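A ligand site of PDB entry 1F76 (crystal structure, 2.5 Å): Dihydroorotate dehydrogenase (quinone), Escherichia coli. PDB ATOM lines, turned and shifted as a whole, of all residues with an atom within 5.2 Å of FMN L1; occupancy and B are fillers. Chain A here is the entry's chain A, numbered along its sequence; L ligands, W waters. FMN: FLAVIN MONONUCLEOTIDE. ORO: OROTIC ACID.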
ATOM      1  N   ALA A  61      21.227  14.432  12.714  1.00  0.00           N
ATOM      2  CA  ALA A  61      21.766  13.115  13.016  1.00  0.00           C
ATOM      3  C   ALA A  61      22.192  12.419  11.719  1.00  0.00           C
ATOM      4  O   ALA A  61      21.724  12.781  10.634  1.00  0.00           O
ATOM      5  CB  ALA A  61      20.731  12.284  13.743  1.00  0.00           C
ATOM      6  N   ALA A  62      23.051  11.420  11.848  1.00  0.00           N
ATOM      7  CA  ALA A  62      23.542  10.670  10.692  1.00  0.00           C
ATOM      8  C   ALA A  62      22.441   9.791  10.095  1.00  0.00           C
ATOM      9  O   ALA A  62      21.488   9.431  10.774  1.00  0.00           O
ATOM     10  CB  ALA A  62      24.729   9.788  11.107  1.00  0.00           C
ATOM     11  N   GLY A  63      22.574   9.467   8.814  1.00  0.00           N
ATOM     12  CA  GLY A  63      21.589   8.633   8.166  1.00  0.00           C
ATOM     13  C   GLY A  63      20.755   9.296   7.090  1.00  0.00           C
ATOM     14  O   GLY A  63      20.215   8.623   6.211  1.00  0.00           O
ATOM     15  N   LYS A  66      23.716  10.329   3.884  1.00  0.00           N
ATOM     16  CA  LYS A  66      24.732   9.292   4.023  1.00  0.00           C
ATOM     17  C   LYS A  66      26.018   9.529   3.241  1.00  0.00           C
ATOM     18  O   LYS A  66      27.099   9.200   3.716  1.00  0.00           O
ATOM     19  CB  LYS A  66      24.114   7.930   3.663  1.00  0.00           C
ATOM     20  CG  LYS A  66      23.148   7.421   4.734  1.00  0.00           C
ATOM     21  CD  LYS A  66      22.145   6.403   4.217  1.00  0.00           C
ATOM     22  CE  LYS A  66      22.364   5.008   4.819  1.00  0.00           C
ATOM     23  NZ  LYS A  66      22.291   4.949   6.319  1.00  0.00           N
ATOM     24  N   GLU A  83      25.874  15.726  10.652  1.00  0.00           N
ATOM     25  CA  GLU A  83      26.622  14.490  10.688  1.00  0.00           C
ATOM     26  C   GLU A  83      26.299  13.675   9.441  1.00  0.00           C
ATOM     27  O   GLU A  83      25.168  13.223   9.252  1.00  0.00           O
ATOM     28  CB  GLU A  83      26.280  13.687  11.957  1.00  0.00           C
ATOM     29  CG  GLU A  83      27.307  12.607  12.320  1.00  0.00           C
ATOM     30  CD  GLU A  83      27.028  11.923  13.660  1.00  0.00           C
ATOM     31  OE1 GLU A  83      26.647  10.741  13.671  1.00  0.00           O
ATOM     32  OE2 GLU A  83      27.186  12.585  14.717  1.00  0.00           O
ATOM     33  N   GLY A  85      27.051  10.387   6.743  1.00  0.00           N
ATOM     34  CA  GLY A  85      27.354   8.981   6.910  1.00  0.00           C
ATOM     35  C   GLY A  85      26.086   8.291   7.385  1.00  0.00           C
ATOM     36  O   GLY A  85      25.024   8.896   7.348  1.00  0.00           O
ATOM     37  N   THR A  86      26.152   7.041   7.855  1.00  0.00           N
ATOM     38  CA  THR A  86      27.366   6.238   7.954  1.00  0.00           C
ATOM     39  C   THR A  86      28.004   5.862   6.614  1.00  0.00           C
ATOM     40  O   THR A  86      27.326   5.424   5.686  1.00  0.00           O
ATOM     41  CB  THR A  86      27.084   4.925   8.718  1.00  0.00           C
ATOM     42  OG1 THR A  86      26.777   5.215  10.085  1.00  0.00           O
ATOM     43  CG2 THR A  86      28.279   3.994   8.663  1.00  0.00           C
ATOM     44  N   LEU A 100      12.487   0.531   4.553  1.00  0.00           N
ATOM     45  CA  LEU A 100      12.090   1.681   5.368  1.00  0.00           C
ATOM     46  C   LEU A 100      10.569   1.724   5.509  1.00  0.00           C
ATOM     47  O   LEU A 100       9.849   1.565   4.525  1.00  0.00           O
ATOM     48  CB  LEU A 100      12.608   2.984   4.737  1.00  0.00           C
ATOM     49  CG  LEU A 100      12.299   4.298   5.451  1.00  0.00           C
ATOM     50  CD1 LEU A 100      12.842   4.276   6.868  1.00  0.00           C
ATOM     51  CD2 LEU A 100      12.906   5.453   4.656  1.00  0.00           C
ATOM     52  N   LEU A 109       9.551   5.621  12.850  1.00  0.00           N
ATOM     53  CA  LEU A 109      10.017   4.935  11.648  1.00  0.00           C
ATOM     54  C   LEU A 109      10.772   3.683  12.056  1.00  0.00           C
ATOM     55  O   LEU A 109      11.310   3.576  13.156  1.00  0.00           O
ATOM     56  CB  LEU A 109      10.979   5.817  10.847  1.00  0.00           C
ATOM     57  CG  LEU A 109      10.562   7.221  10.391  1.00  0.00           C
ATOM     58  CD1 LEU A 109      11.785   7.941   9.857  1.00  0.00           C
ATOM     59  CD2 LEU A 109       9.482   7.135   9.321  1.00  0.00           C
ATOM     60  N   ASN A 111      13.610   1.094  10.167  1.00  0.00           N
ATOM     61  CA  ASN A 111      14.474   0.927   9.013  1.00  0.00           C
ATOM     62  C   ASN A 111      15.490  -0.187   9.210  1.00  0.00           C
ATOM     63  O   ASN A 111      15.851  -0.535  10.349  1.00  0.00           O
ATOM     64  CB  ASN A 111      15.229   2.222   8.695  1.00  0.00           C
ATOM     65  CG  ASN A 111      16.546   2.324   9.450  1.00  0.00           C
ATOM     66  OD1 ASN A 111      17.590   1.710   8.896  1.00  0.00           O
ATOM     67  ND2 ASN A 111      16.625   2.929  10.521  1.00  0.00           N
ATOM     68  N   MET A 113      18.164  -0.285   6.597  1.00  0.00           N
ATOM     69  CA  MET A 113      18.919   0.143   5.423  1.00  0.00           C
ATOM     70  C   MET A 113      20.151  -0.731   5.171  1.00  0.00           C
ATOM     71  O   MET A 113      20.363  -1.207   4.054  1.00  0.00           O
ATOM     72  CB  MET A 113      19.366   1.601   5.582  1.00  0.00           C
ATOM     73  CG  MET A 113      18.248   2.588   5.922  1.00  0.00           C
ATOM     74  SD  MET A 113      16.864   2.727   4.571  1.00  0.00           S
ATOM     75  CE  MET A 113      17.771   3.887   3.332  1.00  0.00           C
ATOM     76  N   PHE A 115      23.569   0.266   5.955  1.00  0.00           N
ATOM     77  CA  PHE A 115      24.689   1.081   5.503  1.00  0.00           C
ATOM     78  C   PHE A 115      24.790   1.233   3.983  1.00  0.00           C
ATOM     79  O   PHE A 115      25.859   1.007   3.402  1.00  0.00           O
ATOM     80  CB  PHE A 115      26.028   0.526   6.026  1.00  0.00           C
ATOM     81  CG  PHE A 115      26.236   0.695   7.505  1.00  0.00           C
ATOM     82  CD1 PHE A 115      25.506   1.637   8.226  1.00  0.00           C
ATOM     83  CD2 PHE A 115      27.191  -0.074   8.174  1.00  0.00           C
ATOM     84  CE1 PHE A 115      25.733   1.821   9.599  1.00  0.00           C
ATOM     85  CE2 PHE A 115      27.435   0.101   9.532  1.00  0.00           C
ATOM     86  CZ  PHE A 115      26.698   1.054  10.259  1.00  0.00           C
ATOM     87  N   ASN A 139      30.461  10.229  10.214  1.00  0.00           N
ATOM     88  CA  ASN A 139      30.085   8.975  10.848  1.00  0.00           C
ATOM     89  C   ASN A 139      30.544   7.800   9.979  1.00  0.00           C
ATOM     90  O   ASN A 139      30.193   7.715   8.806  1.00  0.00           O
ATOM     91  CB  ASN A 139      28.574   8.969  11.055  1.00  0.00           C
ATOM     92  CG  ASN A 139      28.075   7.770  11.802  1.00  0.00           C
ATOM     93  OD1 ASN A 139      28.270   6.635  11.386  1.00  0.00           O
ATOM     94  ND2 ASN A 139      27.416   8.021  12.929  1.00  0.00           N
ATOM     95  N   ASN A 172      30.427   4.433  14.480  1.00  0.00           N
ATOM     96  CA  ASN A 172      29.160   3.724  14.574  1.00  0.00           C
ATOM     97  C   ASN A 172      29.307   2.232  14.856  1.00  0.00           C
ATOM     98  O   ASN A 172      29.634   1.442  13.974  1.00  0.00           O
ATOM     99  CB  ASN A 172      28.333   3.921  13.289  1.00  0.00           C
ATOM    100  CG  ASN A 172      26.950   3.277  13.385  1.00  0.00           C
ATOM    101  OD1 ASN A 172      26.614   2.613  14.372  1.00  0.00           O
ATOM    102  ND2 ASN A 172      26.146   3.463  12.345  1.00  0.00           N
ATOM    103  N   LYS A 217      29.073   6.216  19.003  1.00  0.00           N
ATOM    104  CA  LYS A 217      27.610   6.137  19.015  1.00  0.00           C
ATOM    105  C   LYS A 217      27.102   4.791  19.501  1.00  0.00           C
ATOM    106  O   LYS A 217      27.274   3.765  18.842  1.00  0.00           O
ATOM    107  CB  LYS A 217      27.068   6.426  17.612  1.00  0.00           C
ATOM    108  CG  LYS A 217      25.551   6.621  17.564  1.00  0.00           C
ATOM    109  CD  LYS A 217      25.110   7.215  16.236  1.00  0.00           C
ATOM    110  CE  LYS A 217      23.601   7.436  16.182  1.00  0.00           C
ATOM    111  NZ  LYS A 217      23.200   8.023  14.879  1.00  0.00           N
ATOM    112  N   THR A 245      21.152   8.431  21.439  1.00  0.00           N
ATOM    113  CA  THR A 245      21.330   7.018  21.143  1.00  0.00           C
ATOM    114  C   THR A 245      20.956   6.649  19.693  1.00  0.00           C
ATOM    115  O   THR A 245      20.449   7.486  18.950  1.00  0.00           O
ATOM    116  CB  THR A 245      20.413   6.275  22.144  1.00  0.00           C
ATOM    117  OG1 THR A 245      21.173   5.336  22.905  1.00  0.00           O
ATOM    118  CG2 THR A 245      19.260   5.620  21.431  1.00  0.00           C
ATOM    119  N   ASN A 246      21.202   5.405  19.299  1.00  0.00           N
ATOM    120  CA  ASN A 246      20.860   4.915  17.956  1.00  0.00           C
ATOM    121  C   ASN A 246      19.424   4.377  18.016  1.00  0.00           C
ATOM    122  O   ASN A 246      18.732   4.549  19.018  1.00  0.00           O
ATOM    123  CB  ASN A 246      21.815   3.797  17.523  1.00  0.00           C
ATOM    124  CG  ASN A 246      21.975   3.704  15.999  1.00  0.00           C
ATOM    125  OD1 ASN A 246      20.987   3.613  15.260  1.00  0.00           O
ATOM    126  ND2 ASN A 246      23.220   3.715  15.533  1.00  0.00           N
ATOM    127  N   THR A 247      18.978   3.698  16.968  1.00  0.00           N
ATOM    128  CA  THR A 247      17.611   3.161  16.954  1.00  0.00           C
ATOM    129  C   THR A 247      17.450   1.911  17.822  1.00  0.00           C
ATOM    130  O   THR A 247      18.411   1.202  18.101  1.00  0.00           O
ATOM    131  CB  THR A 247      17.182   2.845  15.530  1.00  0.00           C
ATOM    132  OG1 THR A 247      18.008   1.803  14.998  1.00  0.00           O
ATOM    133  CG2 THR A 247      17.321   4.090  14.681  1.00  0.00           C
ATOM    134  N   SER A 267      12.770   4.407  15.379  1.00  0.00           N
ATOM    135  CA  SER A 267      13.165   5.760  15.739  1.00  0.00           C
ATOM    136  C   SER A 267      11.944   6.654  15.898  1.00  0.00           C
ATOM    137  O   SER A 267      10.812   6.192  15.726  1.00  0.00           O
ATOM    138  CB  SER A 267      14.071   6.352  14.653  1.00  0.00           C
ATOM    139  OG  SER A 267      13.410   6.332  13.396  1.00  0.00           O
ATOM    140  N   GLY A 268      12.171   7.917  16.202  1.00  0.00           N
ATOM    141  CA  GLY A 268      11.051   8.830  16.375  1.00  0.00           C
ATOM    142  C   GLY A 268      10.476   8.829  17.772  1.00  0.00           C
ATOM    143  O   GLY A 268      11.129   8.413  18.729  1.00  0.00           O
ATOM    144  N   LEU A 271      10.913   6.331  20.719  1.00  0.00           N
ATOM    145  CA  LEU A 271      12.274   6.179  21.249  1.00  0.00           C
ATOM    146  C   LEU A 271      12.627   7.313  22.215  1.00  0.00           C
ATOM    147  O   LEU A 271      13.598   7.215  22.963  1.00  0.00           O
ATOM    148  CB  LEU A 271      13.282   6.208  20.084  1.00  0.00           C
ATOM    149  CG  LEU A 271      14.667   5.536  20.087  1.00  0.00           C
ATOM    150  CD1 LEU A 271      15.574   6.307  19.125  1.00  0.00           C
ATOM    151  CD2 LEU A 271      15.289   5.507  21.474  1.00  0.00           C
ATOM    152  N   VAL A 295      20.366  12.150  21.238  1.00  0.00           N
ATOM    153  CA  VAL A 295      19.527  11.984  20.067  1.00  0.00           C
ATOM    154  C   VAL A 295      18.526  10.857  20.303  1.00  0.00           C
ATOM    155  O   VAL A 295      18.831   9.888  20.994  1.00  0.00           O
ATOM    156  CB  VAL A 295      20.385  11.657  18.799  1.00  0.00           C
ATOM    157  CG1 VAL A 295      21.235  10.434  19.060  1.00  0.00           C
ATOM    158  CG2 VAL A 295      19.491  11.423  17.590  1.00  0.00           C
ATOM    159  N   GLY A 296      17.336  10.993  19.726  1.00  0.00           N
ATOM    160  CA  GLY A 296      16.322   9.973  19.885  1.00  0.00           C
ATOM    161  C   GLY A 296      14.956  10.551  20.159  1.00  0.00           C
ATOM    162  O   GLY A 296      14.670  10.990  21.277  1.00  0.00           O
ATOM    163  N   GLY A 297      14.109  10.565  19.136  1.00  0.00           N
ATOM    164  CA  GLY A 297      12.755  11.073  19.284  1.00  0.00           C
ATOM    165  C   GLY A 297      12.556  12.548  19.592  1.00  0.00           C
ATOM    166  O   GLY A 297      11.452  12.936  19.972  1.00  0.00           O
ATOM    167  N   ILE A 298      13.575  13.381  19.446  1.00  0.00           N
ATOM    168  CA  ILE A 298      13.378  14.807  19.712  1.00  0.00           C
ATOM    169  C   ILE A 298      12.444  15.388  18.642  1.00  0.00           C
ATOM    170  O   ILE A 298      12.807  15.404  17.464  1.00  0.00           O
ATOM    171  CB  ILE A 298      14.711  15.578  19.678  1.00  0.00           C
ATOM    172  CG1 ILE A 298      15.612  15.114  20.817  1.00  0.00           C
ATOM    173  CG2 ILE A 298      14.453  17.077  19.778  1.00  0.00           C
ATOM    174  CD1 ILE A 298      16.925  15.870  20.889  1.00  0.00           C
ATOM    175  N   GLN A 316      20.649  16.047  18.414  1.00  0.00           N
ATOM    176  CA  GLN A 316      20.499  15.849  16.984  1.00  0.00           C
ATOM    177  C   GLN A 316      19.078  15.359  16.707  1.00  0.00           C
ATOM    178  O   GLN A 316      18.409  14.826  17.601  1.00  0.00           O
ATOM    179  CB  GLN A 316      21.475  14.781  16.467  1.00  0.00           C
ATOM    180  CG  GLN A 316      22.918  14.945  16.897  1.00  0.00           C
ATOM    181  CD  GLN A 316      23.820  13.900  16.255  1.00  0.00           C
ATOM    182  OE1 GLN A 316      23.477  12.716  16.211  1.00  0.00           O
ATOM    183  NE2 GLN A 316      24.966  14.335  15.756  1.00  0.00           N
ATOM    184  N   ILE A 317      18.620  15.549  15.479  1.00  0.00           N
ATOM    185  CA  ILE A 317      17.296  15.088  15.091  1.00  0.00           C
ATOM    186  C   ILE A 317      17.331  14.398  13.733  1.00  0.00           C
ATOM    187  O   ILE A 317      18.228  14.639  12.924  1.00  0.00           O
ATOM    188  CB  ILE A 317      16.285  16.263  15.005  1.00  0.00           C
ATOM    189  CG1 ILE A 317      16.742  17.260  13.946  1.00  0.00           C
ATOM    190  CG2 ILE A 317      16.141  16.941  16.365  1.00  0.00           C
ATOM    191  CD1 ILE A 317      15.792  18.420  13.739  1.00  0.00           C
ATOM    192  N   TYR A 318      16.359  13.521  13.511  1.00  0.00           N
ATOM    193  CA  TYR A 318      16.235  12.844  12.234  1.00  0.00           C
ATOM    194  C   TYR A 318      14.740  12.650  11.968  1.00  0.00           C
ATOM    195  O   TYR A 318      14.141  13.402  11.194  1.00  0.00           O
ATOM    196  CB  TYR A 318      16.940  11.478  12.243  1.00  0.00           C
ATOM    197  CG  TYR A 318      17.006  10.822  10.874  1.00  0.00           C
ATOM    198  CD1 TYR A 318      15.898  10.839  10.020  1.00  0.00           C
ATOM    199  CD2 TYR A 318      18.160  10.170  10.429  1.00  0.00           C
ATOM    200  CE1 TYR A 318      15.936  10.240   8.766  1.00  0.00           C
ATOM    201  CE2 TYR A 318      18.206   9.565   9.162  1.00  0.00           C
ATOM    202  CZ  TYR A 318      17.085   9.602   8.342  1.00  0.00           C
ATOM    203  OH  TYR A 318      17.093   9.001   7.107  1.00  0.00           O
ATOM    204  N   SER A 319      14.161  11.649  12.614  1.00  0.00           N
ATOM    205  CA  SER A 319      12.750  11.338  12.440  1.00  0.00           C
ATOM    206  C   SER A 319      11.842  12.564  12.578  1.00  0.00           C
ATOM    207  O   SER A 319      10.990  12.829  11.725  1.00  0.00           O
ATOM    208  CB  SER A 319      12.329  10.270  13.435  1.00  0.00           C
ATOM    209  OG  SER A 319      13.064   9.077  13.211  1.00  0.00           O
ATOM    210  N   GLY A 320      12.033  13.326  13.656  1.00  0.00           N
ATOM    211  CA  GLY A 320      11.232  14.506  13.898  1.00  0.00           C
ATOM    212  C   GLY A 320      11.347  15.525  12.783  1.00  0.00           C
ATOM    213  O   GLY A 320      10.417  16.291  12.533  1.00  0.00           O
HETATM  214  N1  FMN L   1      22.576   6.377  12.471  1.00  0.00           N
HETATM  215  C2  FMN L   1      23.939   6.267  12.159  1.00  0.00           C
HETATM  216  O2  FMN L   1      24.732   6.442  13.044  1.00  0.00           O
HETATM  217  N3  FMN L   1      24.282   5.955  10.806  1.00  0.00           N
HETATM  218  C4  FMN L   1      23.298   5.759   9.811  1.00  0.00           C
HETATM  219  O4  FMN L   1      23.629   5.471   8.651  1.00  0.00           O
HETATM  220  C4A FMN L   1      21.898   5.860  10.267  1.00  0.00           C
HETATM  221  N5  FMN L   1      20.900   5.699   9.209  1.00  0.00           N
HETATM  222  C5A FMN L   1      19.692   6.010   9.478  1.00  0.00           C
HETATM  223  C6  FMN L   1      18.694   5.943   8.467  1.00  0.00           C
HETATM  224  C7  FMN L   1      17.324   6.065   8.785  1.00  0.00           C
HETATM  225  C7M FMN L   1      16.186   5.933   7.702  1.00  0.00           C
HETATM  226  C8  FMN L   1      16.907   6.273  10.145  1.00  0.00           C
HETATM  227  C8M FMN L   1      15.433   6.408  10.589  1.00  0.00           C
HETATM  228  C9  FMN L   1      17.874   6.343  11.166  1.00  0.00           C
HETATM  229  C9A FMN L   1      19.229   6.233  10.877  1.00  0.00           C
HETATM  230  N10 FMN L   1      20.171   6.340  11.989  1.00  0.00           N
HETATM  231  C10 FMN L   1      21.520   6.227  11.614  1.00  0.00           C
HETATM  232  C1' FMN L   1      19.829   6.596  13.294  1.00  0.00           C
HETATM  233  C2' FMN L   1      19.750   8.153  13.622  1.00  0.00           C
HETATM  234  O2' FMN L   1      20.974   8.868  13.300  1.00  0.00           O
HETATM  235  C3' FMN L   1      19.306   8.354  15.081  1.00  0.00           C
HETATM  236  O3' FMN L   1      20.417   7.930  15.846  1.00  0.00           O
HETATM  237  C4' FMN L   1      17.901   7.642  15.512  1.00  0.00           C
HETATM  238  O4' FMN L   1      17.023   7.547  14.368  1.00  0.00           O
HETATM  239  C5' FMN L   1      17.356   8.389  16.647  1.00  0.00           C
HETATM  240  O5' FMN L   1      16.942   9.766  16.376  1.00  0.00           O
HETATM  241  P   FMN L   1      15.477  10.168  15.775  1.00  0.00           P
HETATM  242  O1P FMN L   1      15.436  11.651  16.062  1.00  0.00           O
HETATM  243  O2P FMN L   1      15.364   9.675  14.425  1.00  0.00           O
HETATM  244  O3P FMN L   1      14.445   9.537  16.724  1.00  0.00           O
HETATM  245  N1  ORO L   2      19.978   2.074  10.522  1.00  0.00           N
HETATM  246  C2  ORO L   2      19.794   2.528  11.842  1.00  0.00           C
HETATM  247  O2  ORO L   2      18.678   2.614  12.375  1.00  0.00           O
HETATM  248  N3  ORO L   2      20.978   2.858  12.497  1.00  0.00           N
HETATM  249  C4  ORO L   2      22.280   2.795  11.981  1.00  0.00           C
HETATM  250  O4  ORO L   2      23.252   3.117  12.649  1.00  0.00           O
HETATM  251  C5  ORO L   2      22.392   2.319  10.601  1.00  0.00           C
HETATM  252  C6  ORO L   2      21.248   1.988   9.926  1.00  0.00           C
HETATM  253  C7  ORO L   2      21.282   1.477   8.490  1.00  0.00           C
HETATM  254  O71 ORO L   2      21.866   2.202   7.635  1.00  0.00           O
HETATM  255  O72 ORO L   2      20.725   0.377   8.304  1.00  0.00           O
HETATM  256  O   HOH W   1      13.534  13.391  15.853  1.00  0.00           O
HETATM  257  O   HOH W   2      14.083   4.024  11.913  1.00  0.00           O
HETATM  258  O   HOH W   3      16.374  13.039  18.053  1.00  0.00           O
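N of Gly 268 lies within hydrogen-bond range of O3P of FMN L1, 2.8 Å away.
An oxygen (O4) of FMN L1 sits at hydrogen-bond distance from the side-chain amino group (NZ) of Lys 66.
The side-chain hydroxyl of Ser 319 is in hydrogen-bond range of an oxygen (O2P) of FMN L1 (2.7 Å).
ND2 of Asn 111 lies within hydrogen-bond range of O2 of ORO L2 (2.8 Å).
The backbone NH (N) of Thr 86 sits at hydrogen-bond distance from an oxygen (O4) of FMN L1.
The backbone carbonyl oxygen of Thr 245 lies within hydrogen-bond range of an oxygen (O3') of FMN L1.
NZ of Lys 66 is in salt-bridge range of O71 of ORO L2 (3.1 Å).
O1P of FMN L1 lies within hydrogen-bond range of N of Tyr 318 (3.3 Å).
The backbone NH (N) of Gly 297 lies within hydrogen-bond range of an oxygen (O3P) of FMN L1 (2.6 Å).
The side-chain hydroxyl (OG1) of Thr 247 is in hydrogen-bond range of an oxygen (O2) of ORO L2.
O of Ala 62 sits at hydrogen-bond distance from O2' of FMN L1 (2.6 Å).
A nitrogen (N3) of ORO L2 sits at hydrogen-bond distance from the side-chain amide oxygen of Asn 246 (2.9 Å).
NZ of Lys 217 lies within hydrogen-bond range of O2' of FMN L1 (2.9 Å).
The side-chain amide nitrogen (ND2) of Asn 172 is in hydrogen-bond range of an oxygen (O2) of FMN L1 (3.4 Å).
The side-chain hydroxyl (OG1) of Thr 86 is in hydrogen-bond range of a nitrogen (N3) of FMN L1 (2.7 Å).
N of Ser 319 sits at hydrogen-bond distance from O2P of FMN L1.
ND2 of Asn 139 lies within hydrogen-bond range of O2 of FMN L1.
N of Met 113 sits at hydrogen-bond distance from O72 of ORO L2 (3.1 Å).
The side-chain amide nitrogen (ND2) of Asn 172 sits at hydrogen-bond distance from an oxygen (O4) of ORO L2.
N of Phe 115 lies within hydrogen-bond range of O71 of ORO L2, at 3.1 Å.
The backbone NH (N) of Gly 63 sits at hydrogen-bond distance from the backbone carbonyl oxygen (O) of Gly 85, 2.9 Å away.
O of Val 295 sits at hydrogen-bond distance from N of Thr 245.
The side-chain hydroxyl of Ser 319 sits at hydrogen-bond distance from the side-chain hydroxyl of Ser 267, 2.8 Å away.
The backbone NH of Met 113 is in hydrogen-bond range of the side-chain amide oxygen of Asn 111, at 3.1 Å.
The side-chain hydroxyl (OG1) of Thr 247 lies within hydrogen-bond range of the side-chain amide oxygen (OD1) of Asn 246.
The backbone carbonyl oxygen (O) of Gly 63 is in hydrogen-bond range of the side-chain hydroxyl (OH) of Tyr 318, at 3.3 Å.
ND2 of Asn 139 is in hydrogen-bond range of OE1 of Glu 83, 2.9 Å away.
The backbone NH (N) of Gly 268 is in hydrogen-bond range of the side-chain hydroxyl (OG) of Ser 319, 3.3 Å away.
Residues that only touch FMN L1: Gly 63, Ser 267, Val 295, Asn 111, Ala 61, Thr 247, Gly 296, Leu 271, Asn 246, Leu 100 and Gly 85.
Of the 30 residues printed, 22 come within 4 Å of FMN L1.
Along chain A the residues within 4 Å of FMN L1 span positions 61 to 319.
Water W1 lies within hydrogen-bond range of an oxygen (O1P) of FMN L1 (2.6 Å), the backbone NH of Gly 320 (2.7 Å) and the backbone carbonyl oxygen of Ile 298 (2.7 Å).
Water W3 lies within hydrogen-bond range of O1P of FMN L1 (2.6 Å), O of Gln 316 (2.7 Å), N of Gly 296 (2.8 Å) and N of Ile 298 (3.1 Å).
Water W2 lies within hydrogen-bond range of OG of Ser 267, O of Leu 109 and ND2 of Asn 111.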
